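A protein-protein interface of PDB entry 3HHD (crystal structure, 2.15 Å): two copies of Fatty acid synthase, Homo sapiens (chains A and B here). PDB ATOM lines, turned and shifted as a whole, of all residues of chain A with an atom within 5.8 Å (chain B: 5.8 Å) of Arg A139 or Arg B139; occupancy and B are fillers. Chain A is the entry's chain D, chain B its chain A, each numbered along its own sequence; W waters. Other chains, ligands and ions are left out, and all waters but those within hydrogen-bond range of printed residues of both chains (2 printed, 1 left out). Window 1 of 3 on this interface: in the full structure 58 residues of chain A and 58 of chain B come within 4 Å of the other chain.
Gln A138 touches Ser B114 (OE1 to O, 3.8 Å). Arg A139 touches Arg B139 (CZ to NE, 3.6 Å). CB of Arg A139 touches OD2 of Asp B160 (3.4 Å). Ala A140 touches Asp B160 (CB to OD1, 3.6 Å). CB of Arg B139 touches OD2 of Asp A160 (3.4 Å). Asp A160 touches Ala B140.
Water W1 bridges O of Ala A140 and O of Asp B160. Water W2 lies within hydrogen-bond range of O of Ala A158 (3.1 Å), O of Ala B158 (3.3 Å), N of Asp B160 (3.4 Å) and N of Asp A160 (3.4 Å).
The side-chain amide nitrogen (NE2) of Gln B138 sits close to the backbone NH (N) of Ala B140 (3.1 Å). The guanidinium group (NH1) of Arg B139 lies within salt-bridge range of the side-chain carboxylate (OD2) of Asp B160, 2.9 Å away. OD2 of Asp A160 is in salt-bridge range of NH1 of Arg A139. NH2 of Arg A139 lies within hydrogen-bond range of O of Ser A114 (3.1 Å). O of Ser B114 is in hydrogen-bond range of NH2 of Arg B139 (3.1 Å).
Arg B139 touches just these residues of chain A: Arg A139 and Asp A160. Of the printed residues of chain A, Gln B138 touches Asp A160. Of the printed residues of chain B, Gln A138 touches Ser B114 (3.8 Å) and Asp B160 (3.1 Å). Met B142 touches none of the printed residues of chain A. The nearest residue of chain B that does not touch Arg A139 is Ser B116 (4.9 Å). The nearest residue of chain A that does not touch Arg B139 is Ser A116 (4.9 Å).
The side-chain amide nitrogen (NE2) of Gln B138 lies within hydrogen-bond range of the side-chain carboxylate (OD1) of Asp A160, at 3.0 Å. The side-chain carboxylate of Asp B160 sits at hydrogen-bond distance from the side-chain amide nitrogen of Gln A138, at 3.1 Å. N of Asp B160 lies within hydrogen-bond range of O of Ala A158, 3.0 Å away. O of Ala B158 lies within hydrogen-bond range of N of Asp A160, at 3.0 Å.
Of the 13 printed residues of chain A, 5 touch a printed residue of chain B. Hydrophobic or aromatic side chains of chain A within 4 Å of the printed part of chain B: Ala A140 and Ala A158. Along chain A the printed residues that touch a printed residue of chain B span positions 138 to 160. Of the 13 printed residues of chain B, 6 touch a printed residue of chain A. Among the printed residues, 10 pairs touch across the chains.
Gln A138 touches Asp B160, and with the chains exchanged Asp A160 touches Gln B138. Arg B139 touches its own counterpart, Arg A139. Arg A139 touches Asp B160, and with the chains exchanged Asp A160 touches Arg B139. Ala A158 touches Asp B160, and with the chains exchanged Asp A160 touches Ala B158. Positions printed for both chains: 113, 114, 115, 116, 137, 138, 139, 140, 141, 142, 143, 158 and 160. Of the 10 pairs that touch across the chains among the printed residues, 9 have their exchanged pair printed and touching as well.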
ATOM      1  N   VAL A 113       8.102 -15.495 -26.766  1.00  0.00           N
ATOM      2  CA  VAL A 113       9.559 -15.628 -26.670  1.00  0.00           C
ATOM      3  C   VAL A 113       9.936 -15.928 -25.219  1.00  0.00           C
ATOM      4  O   VAL A 113       9.323 -15.388 -24.294  1.00  0.00           O
ATOM      5  CB  VAL A 113      10.286 -14.357 -27.189  1.00  0.00           C
ATOM      6  CG1 VAL A 113       9.698 -13.104 -26.543  1.00  0.00           C
ATOM      7  CG2 VAL A 113      11.858 -14.450 -26.907  1.00  0.00           C
ATOM      8  N   SER A 114      10.948 -16.761 -25.023  1.00  0.00           N
ATOM      9  CA  SER A 114      11.352 -17.136 -23.662  1.00  0.00           C
ATOM     10  C   SER A 114      12.835 -16.954 -23.319  1.00  0.00           C
ATOM     11  O   SER A 114      13.226 -17.025 -22.171  1.00  0.00           O
ATOM     12  CB  SER A 114      10.874 -18.564 -23.342  1.00  0.00           C
ATOM     13  OG  SER A 114      11.618 -19.491 -24.120  1.00  0.00           O
ATOM     14  N   GLY A 115      13.658 -16.668 -24.309  1.00  0.00           N
ATOM     15  CA  GLY A 115      15.069 -16.492 -24.056  1.00  0.00           C
ATOM     16  C   GLY A 115      15.662 -15.210 -24.615  1.00  0.00           C
ATOM     17  O   GLY A 115      15.241 -14.695 -25.660  1.00  0.00           O
ATOM     18  N   SER A 116      16.648 -14.694 -23.896  1.00  0.00           N
ATOM     19  CA  SER A 116      17.352 -13.471 -24.289  1.00  0.00           C
ATOM     20  C   SER A 116      18.864 -13.722 -24.116  1.00  0.00           C
ATOM     21  O   SER A 116      19.570 -12.936 -23.468  1.00  0.00           O
ATOM     22  CB  SER A 116      16.907 -12.306 -23.390  1.00  0.00           C
ATOM     23  OG  SER A 116      15.864 -11.558 -24.000  1.00  0.00           O
ATOM     24  N   CYS A 137      18.344  -6.450 -28.632  1.00  0.00           N
ATOM     25  CA  CYS A 137      18.221  -7.683 -27.874  1.00  0.00           C
ATOM     26  C   CYS A 137      17.183  -7.712 -26.747  1.00  0.00           C
ATOM     27  O   CYS A 137      16.820  -8.798 -26.300  1.00  0.00           O
ATOM     28  CB  CYS A 137      19.596  -8.063 -27.292  1.00  0.00           C
ATOM     29  SG  CYS A 137      20.878  -8.231 -28.543  1.00  0.00           S
ATOM     30  N   GLN A 138      16.753  -6.549 -26.248  1.00  0.00           N
ATOM     31  CA  GLN A 138      15.815  -6.539 -25.119  1.00  0.00           C
ATOM     32  C   GLN A 138      14.528  -7.254 -25.563  1.00  0.00           C
ATOM     33  O   GLN A 138      14.127  -7.175 -26.721  1.00  0.00           O
ATOM     34  CB  GLN A 138      15.524  -5.123 -24.620  1.00  0.00           C
ATOM     35  CG  GLN A 138      14.022  -4.861 -24.378  1.00  0.00           C
ATOM     36  CD  GLN A 138      13.549  -5.236 -22.959  1.00  0.00           C
ATOM     37  OE1 GLN A 138      14.204  -6.002 -22.248  1.00  0.00           O
ATOM     38  NE2 GLN A 138      12.403  -4.697 -22.557  1.00  0.00           N
ATOM     39  N   ARG A 139      13.925  -8.025 -24.670  1.00  0.00           N
ATOM     40  CA  ARG A 139      12.750  -8.816 -25.044  1.00  0.00           C
ATOM     41  C   ARG A 139      11.594  -8.070 -25.719  1.00  0.00           C
ATOM     42  O   ARG A 139      11.085  -8.527 -26.719  1.00  0.00           O
ATOM     43  CB  ARG A 139      12.249  -9.675 -23.893  1.00  0.00           C
ATOM     44  CG  ARG A 139      11.907 -11.058 -24.389  1.00  0.00           C
ATOM     45  CD  ARG A 139      11.535 -11.969 -23.290  1.00  0.00           C
ATOM     46  NE  ARG A 139      12.699 -12.540 -22.627  1.00  0.00           N
ATOM     47  CZ  ARG A 139      12.609 -13.601 -21.848  1.00  0.00           C
ATOM     48  NH1 ARG A 139      11.421 -14.151 -21.711  1.00  0.00           N
ATOM     49  NH2 ARG A 139      13.669 -14.084 -21.203  1.00  0.00           N
ATOM     50  N   ALA A 140      11.254  -6.889 -25.222  1.00  0.00           N
ATOM     51  CA  ALA A 140      10.182  -6.096 -25.793  1.00  0.00           C
ATOM     52  C   ALA A 140      10.441  -5.755 -27.247  1.00  0.00           C
ATOM     53  O   ALA A 140       9.484  -5.609 -28.018  1.00  0.00           O
ATOM     54  CB  ALA A 140       9.971  -4.813 -24.992  1.00  0.00           C
ATOM     55  N   MET A 141      11.714  -5.596 -27.610  1.00  0.00           N
ATOM     56  CA  MET A 141      12.067  -5.254 -29.009  1.00  0.00           C
ATOM     57  C   MET A 141      11.728  -6.364 -30.015  1.00  0.00           C
ATOM     58  O   MET A 141      11.565  -6.085 -31.213  1.00  0.00           O
ATOM     59  CB  MET A 141      13.564  -4.906 -29.171  1.00  0.00           C
ATOM     60  CG  MET A 141      14.052  -3.665 -28.396  1.00  0.00           C
ATOM     61  SD  MET A 141      13.193  -2.130 -28.864  1.00  0.00           S
ATOM     62  CE  MET A 141      12.340  -1.985 -27.275  1.00  0.00           C
ATOM     63  N   MET A 142      11.624  -7.615 -29.550  1.00  0.00           N
ATOM     64  CA  MET A 142      11.267  -8.730 -30.452  1.00  0.00           C
ATOM     65  C   MET A 142       9.916  -8.412 -31.055  1.00  0.00           C
ATOM     66  O   MET A 142       9.632  -8.782 -32.177  1.00  0.00           O
ATOM     67  CB  MET A 142      11.176 -10.064 -29.687  1.00  0.00           C
ATOM     68  CG  MET A 142      12.480 -10.448 -28.928  1.00  0.00           C
ATOM     69  SD  MET A 142      13.923 -10.652 -30.058  1.00  0.00           S
ATOM     70  CE  MET A 142      14.894  -9.145 -29.701  1.00  0.00           C
ATOM     71  N   ALA A 143       9.078  -7.683 -30.325  1.00  0.00           N
ATOM     72  CA  ALA A 143       7.777  -7.243 -30.904  1.00  0.00           C
ATOM     73  C   ALA A 143       7.867  -5.811 -31.420  1.00  0.00           C
ATOM     74  O   ALA A 143       7.376  -5.497 -32.502  1.00  0.00           O
ATOM     75  CB  ALA A 143       6.649  -7.345 -29.875  1.00  0.00           C
ATOM     76  N   ALA A 158       5.536  -8.631 -26.260  1.00  0.00           N
ATOM     77  CA  ALA A 158       6.325  -9.852 -26.225  1.00  0.00           C
ATOM     78  C   ALA A 158       5.794 -10.598 -24.971  1.00  0.00           C
ATOM     79  O   ALA A 158       5.684 -10.050 -23.889  1.00  0.00           O
ATOM     80  CB  ALA A 158       7.844  -9.531 -26.049  1.00  0.00           C
ATOM     81  N   ASP A 160       5.673 -14.202 -22.404  1.00  0.00           N
ATOM     82  CA  ASP A 160       6.319 -15.444 -22.013  1.00  0.00           C
ATOM     83  C   ASP A 160       5.393 -16.256 -21.122  1.00  0.00           C
ATOM     84  O   ASP A 160       5.044 -15.817 -20.006  1.00  0.00           O
ATOM     85  CB  ASP A 160       7.616 -15.135 -21.231  1.00  0.00           C
ATOM     86  CG  ASP A 160       8.517 -16.388 -21.046  1.00  0.00           C
ATOM     87  OD1 ASP A 160       8.033 -17.533 -21.281  1.00  0.00           O
ATOM     88  OD2 ASP A 160       9.707 -16.240 -20.639  1.00  0.00           O
ATOM     89  N   VAL B 113       7.109  -7.380 -16.559  1.00  0.00           N
ATOM     90  CA  VAL B 113       8.502  -7.640 -16.091  1.00  0.00           C
ATOM     91  C   VAL B 113       9.464  -7.559 -17.281  1.00  0.00           C
ATOM     92  O   VAL B 113       9.112  -7.991 -18.373  1.00  0.00           O
ATOM     93  CB  VAL B 113       8.632  -9.069 -15.379  1.00  0.00           C
ATOM     94  CG1 VAL B 113       8.030 -10.158 -16.298  1.00  0.00           C
ATOM     95  CG2 VAL B 113      10.130  -9.380 -15.029  1.00  0.00           C
ATOM     96  N   SER B 114      10.682  -7.046 -17.068  1.00  0.00           N
ATOM     97  CA  SER B 114      11.641  -6.920 -18.161  1.00  0.00           C
ATOM     98  C   SER B 114      13.037  -7.487 -17.872  1.00  0.00           C
ATOM     99  O   SER B 114      13.866  -7.570 -18.758  1.00  0.00           O
ATOM    100  CB  SER B 114      11.771  -5.457 -18.592  1.00  0.00           C
ATOM    101  OG  SER B 114      12.406  -4.696 -17.575  1.00  0.00           O
ATOM    102  N   GLY B 115      13.297  -7.909 -16.648  1.00  0.00           N
ATOM    103  CA  GLY B 115      14.604  -8.439 -16.322  1.00  0.00           C
ATOM    104  C   GLY B 115      14.602  -9.808 -15.667  1.00  0.00           C
ATOM    105  O   GLY B 115      13.710 -10.144 -14.900  1.00  0.00           O
ATOM    106  N   SER B 116      15.624 -10.596 -16.001  1.00  0.00           N
ATOM    107  CA  SER B 116      15.804 -11.938 -15.479  1.00  0.00           C
ATOM    108  C   SER B 116      17.288 -12.084 -15.087  1.00  0.00           C
ATOM    109  O   SER B 116      17.971 -13.053 -15.483  1.00  0.00           O
ATOM    110  CB  SER B 116      15.420 -12.966 -16.563  1.00  0.00           C
ATOM    111  OG  SER B 116      14.075 -13.433 -16.395  1.00  0.00           O
ATOM    112  N   CYS B 137      13.157 -18.803 -11.515  1.00  0.00           N
ATOM    113  CA  CYS B 137      13.652 -17.602 -12.182  1.00  0.00           C
ATOM    114  C   CYS B 137      13.159 -17.323 -13.597  1.00  0.00           C
ATOM    115  O   CYS B 137      13.264 -16.195 -14.075  1.00  0.00           O
ATOM    116  CB  CYS B 137      15.181 -17.589 -12.179  1.00  0.00           C
ATOM    117  SG  CYS B 137      15.892 -17.713 -10.544  1.00  0.00           S
ATOM    118  N   GLN B 138      12.732 -18.350 -14.306  1.00  0.00           N
ATOM    119  CA  GLN B 138      12.266 -18.192 -15.681  1.00  0.00           C
ATOM    120  C   GLN B 138      11.084 -17.181 -15.700  1.00  0.00           C
ATOM    121  O   GLN B 138      10.235 -17.166 -14.818  1.00  0.00           O
ATOM    122  CB  GLN B 138      11.858 -19.563 -16.257  1.00  0.00           C
ATOM    123  CG  GLN B 138      10.523 -19.552 -16.995  1.00  0.00           C
ATOM    124  CD  GLN B 138      10.656 -19.087 -18.429  1.00  0.00           C
ATOM    125  OE1 GLN B 138      11.764 -18.956 -18.944  1.00  0.00           O
ATOM    126  NE2 GLN B 138       9.528 -18.826 -19.080  1.00  0.00           N
ATOM    127  N   ARG B 139      11.093 -16.281 -16.671  1.00  0.00           N
ATOM    128  CA  ARG B 139      10.124 -15.200 -16.733  1.00  0.00           C
ATOM    129  C   ARG B 139       8.662 -15.568 -16.569  1.00  0.00           C
ATOM    130  O   ARG B 139       7.948 -14.916 -15.839  1.00  0.00           O
ATOM    131  CB  ARG B 139      10.344 -14.293 -17.957  1.00  0.00           C
ATOM    132  CG  ARG B 139      10.265 -12.844 -17.555  1.00  0.00           C
ATOM    133  CD  ARG B 139      10.586 -11.940 -18.654  1.00  0.00           C
ATOM    134  NE  ARG B 139      12.013 -11.723 -18.791  1.00  0.00           N
ATOM    135  CZ  ARG B 139      12.502 -10.711 -19.482  1.00  0.00           C
ATOM    136  NH1 ARG B 139      11.658  -9.861 -20.022  1.00  0.00           N
ATOM    137  NH2 ARG B 139      13.802 -10.554 -19.639  1.00  0.00           N
ATOM    138  N   ALA B 140       8.235 -16.648 -17.213  1.00  0.00           N
ATOM    139  CA  ALA B 140       6.857 -17.059 -17.137  1.00  0.00           C
ATOM    140  C   ALA B 140       6.434 -17.365 -15.714  1.00  0.00           C
ATOM    141  O   ALA B 140       5.264 -17.194 -15.376  1.00  0.00           O
ATOM    142  CB  ALA B 140       6.565 -18.247 -18.057  1.00  0.00           C
ATOM    143  N   MET B 141       7.367 -17.837 -14.900  1.00  0.00           N
ATOM    144  CA  MET B 141       7.066 -18.179 -13.494  1.00  0.00           C
ATOM    145  C   MET B 141       6.660 -16.996 -12.636  1.00  0.00           C
ATOM    146  O   MET B 141       5.965 -17.173 -11.629  1.00  0.00           O
ATOM    147  CB  MET B 141       8.233 -18.931 -12.845  1.00  0.00           C
ATOM    148  CG  MET B 141       8.575 -20.286 -13.568  1.00  0.00           C
ATOM    149  SD  MET B 141       7.257 -21.564 -13.257  1.00  0.00           S
ATOM    150  CE  MET B 141       7.401 -22.514 -14.737  1.00  0.00           C
ATOM    151  N   MET B 142       7.106 -15.793 -13.023  1.00  0.00           N
ATOM    152  CA  MET B 142       6.758 -14.567 -12.285  1.00  0.00           C
ATOM    153  C   MET B 142       5.238 -14.480 -12.240  1.00  0.00           C
ATOM    154  O   MET B 142       4.695 -13.988 -11.290  1.00  0.00           O
ATOM    155  CB  MET B 142       7.335 -13.305 -12.967  1.00  0.00           C
ATOM    156  CG  MET B 142       8.868 -13.333 -13.148  1.00  0.00           C
ATOM    157  SD  MET B 142       9.715 -13.435 -11.550  1.00  0.00           S
ATOM    158  CE  MET B 142      10.390 -15.217 -11.616  1.00  0.00           C
ATOM    159  N   ALA B 143       4.565 -14.989 -13.264  1.00  0.00           N
ATOM    160  CA  ALA B 143       3.097 -15.033 -13.268  1.00  0.00           C
ATOM    161  C   ALA B 143       2.603 -16.427 -12.843  1.00  0.00           C
ATOM    162  O   ALA B 143       1.674 -16.561 -12.066  1.00  0.00           O
ATOM    163  CB  ALA B 143       2.551 -14.700 -14.696  1.00  0.00           C
ATOM    164  N   ALA B 158       3.249 -13.368 -18.346  1.00  0.00           N
ATOM    165  CA  ALA B 158       4.307 -12.407 -18.028  1.00  0.00           C
ATOM    166  C   ALA B 158       4.510 -11.618 -19.335  1.00  0.00           C
ATOM    167  O   ALA B 158       4.610 -12.175 -20.442  1.00  0.00           O
ATOM    168  CB  ALA B 158       5.646 -13.115 -17.613  1.00  0.00           C
ATOM    169  N   ASP B 160       6.253  -8.204 -21.574  1.00  0.00           N
ATOM    170  CA  ASP B 160       7.332  -7.207 -21.604  1.00  0.00           C
ATOM    171  C   ASP B 160       7.061  -6.229 -22.743  1.00  0.00           C
ATOM    172  O   ASP B 160       7.031  -6.614 -23.925  1.00  0.00           O
ATOM    173  CB  ASP B 160       8.684  -7.913 -21.861  1.00  0.00           C
ATOM    174  CG  ASP B 160       9.886  -6.998 -21.628  1.00  0.00           C
ATOM    175  OD1 ASP B 160       9.695  -5.749 -21.537  1.00  0.00           O
ATOM    176  OD2 ASP B 160      11.029  -7.536 -21.557  1.00  0.00           O
HETATM  177  O   HOH W   1       6.822  -5.195 -26.790  1.00  0.00           O
HETATM  178  O   HOH W   2       7.501 -11.360 -21.785  1.00  0.00           O
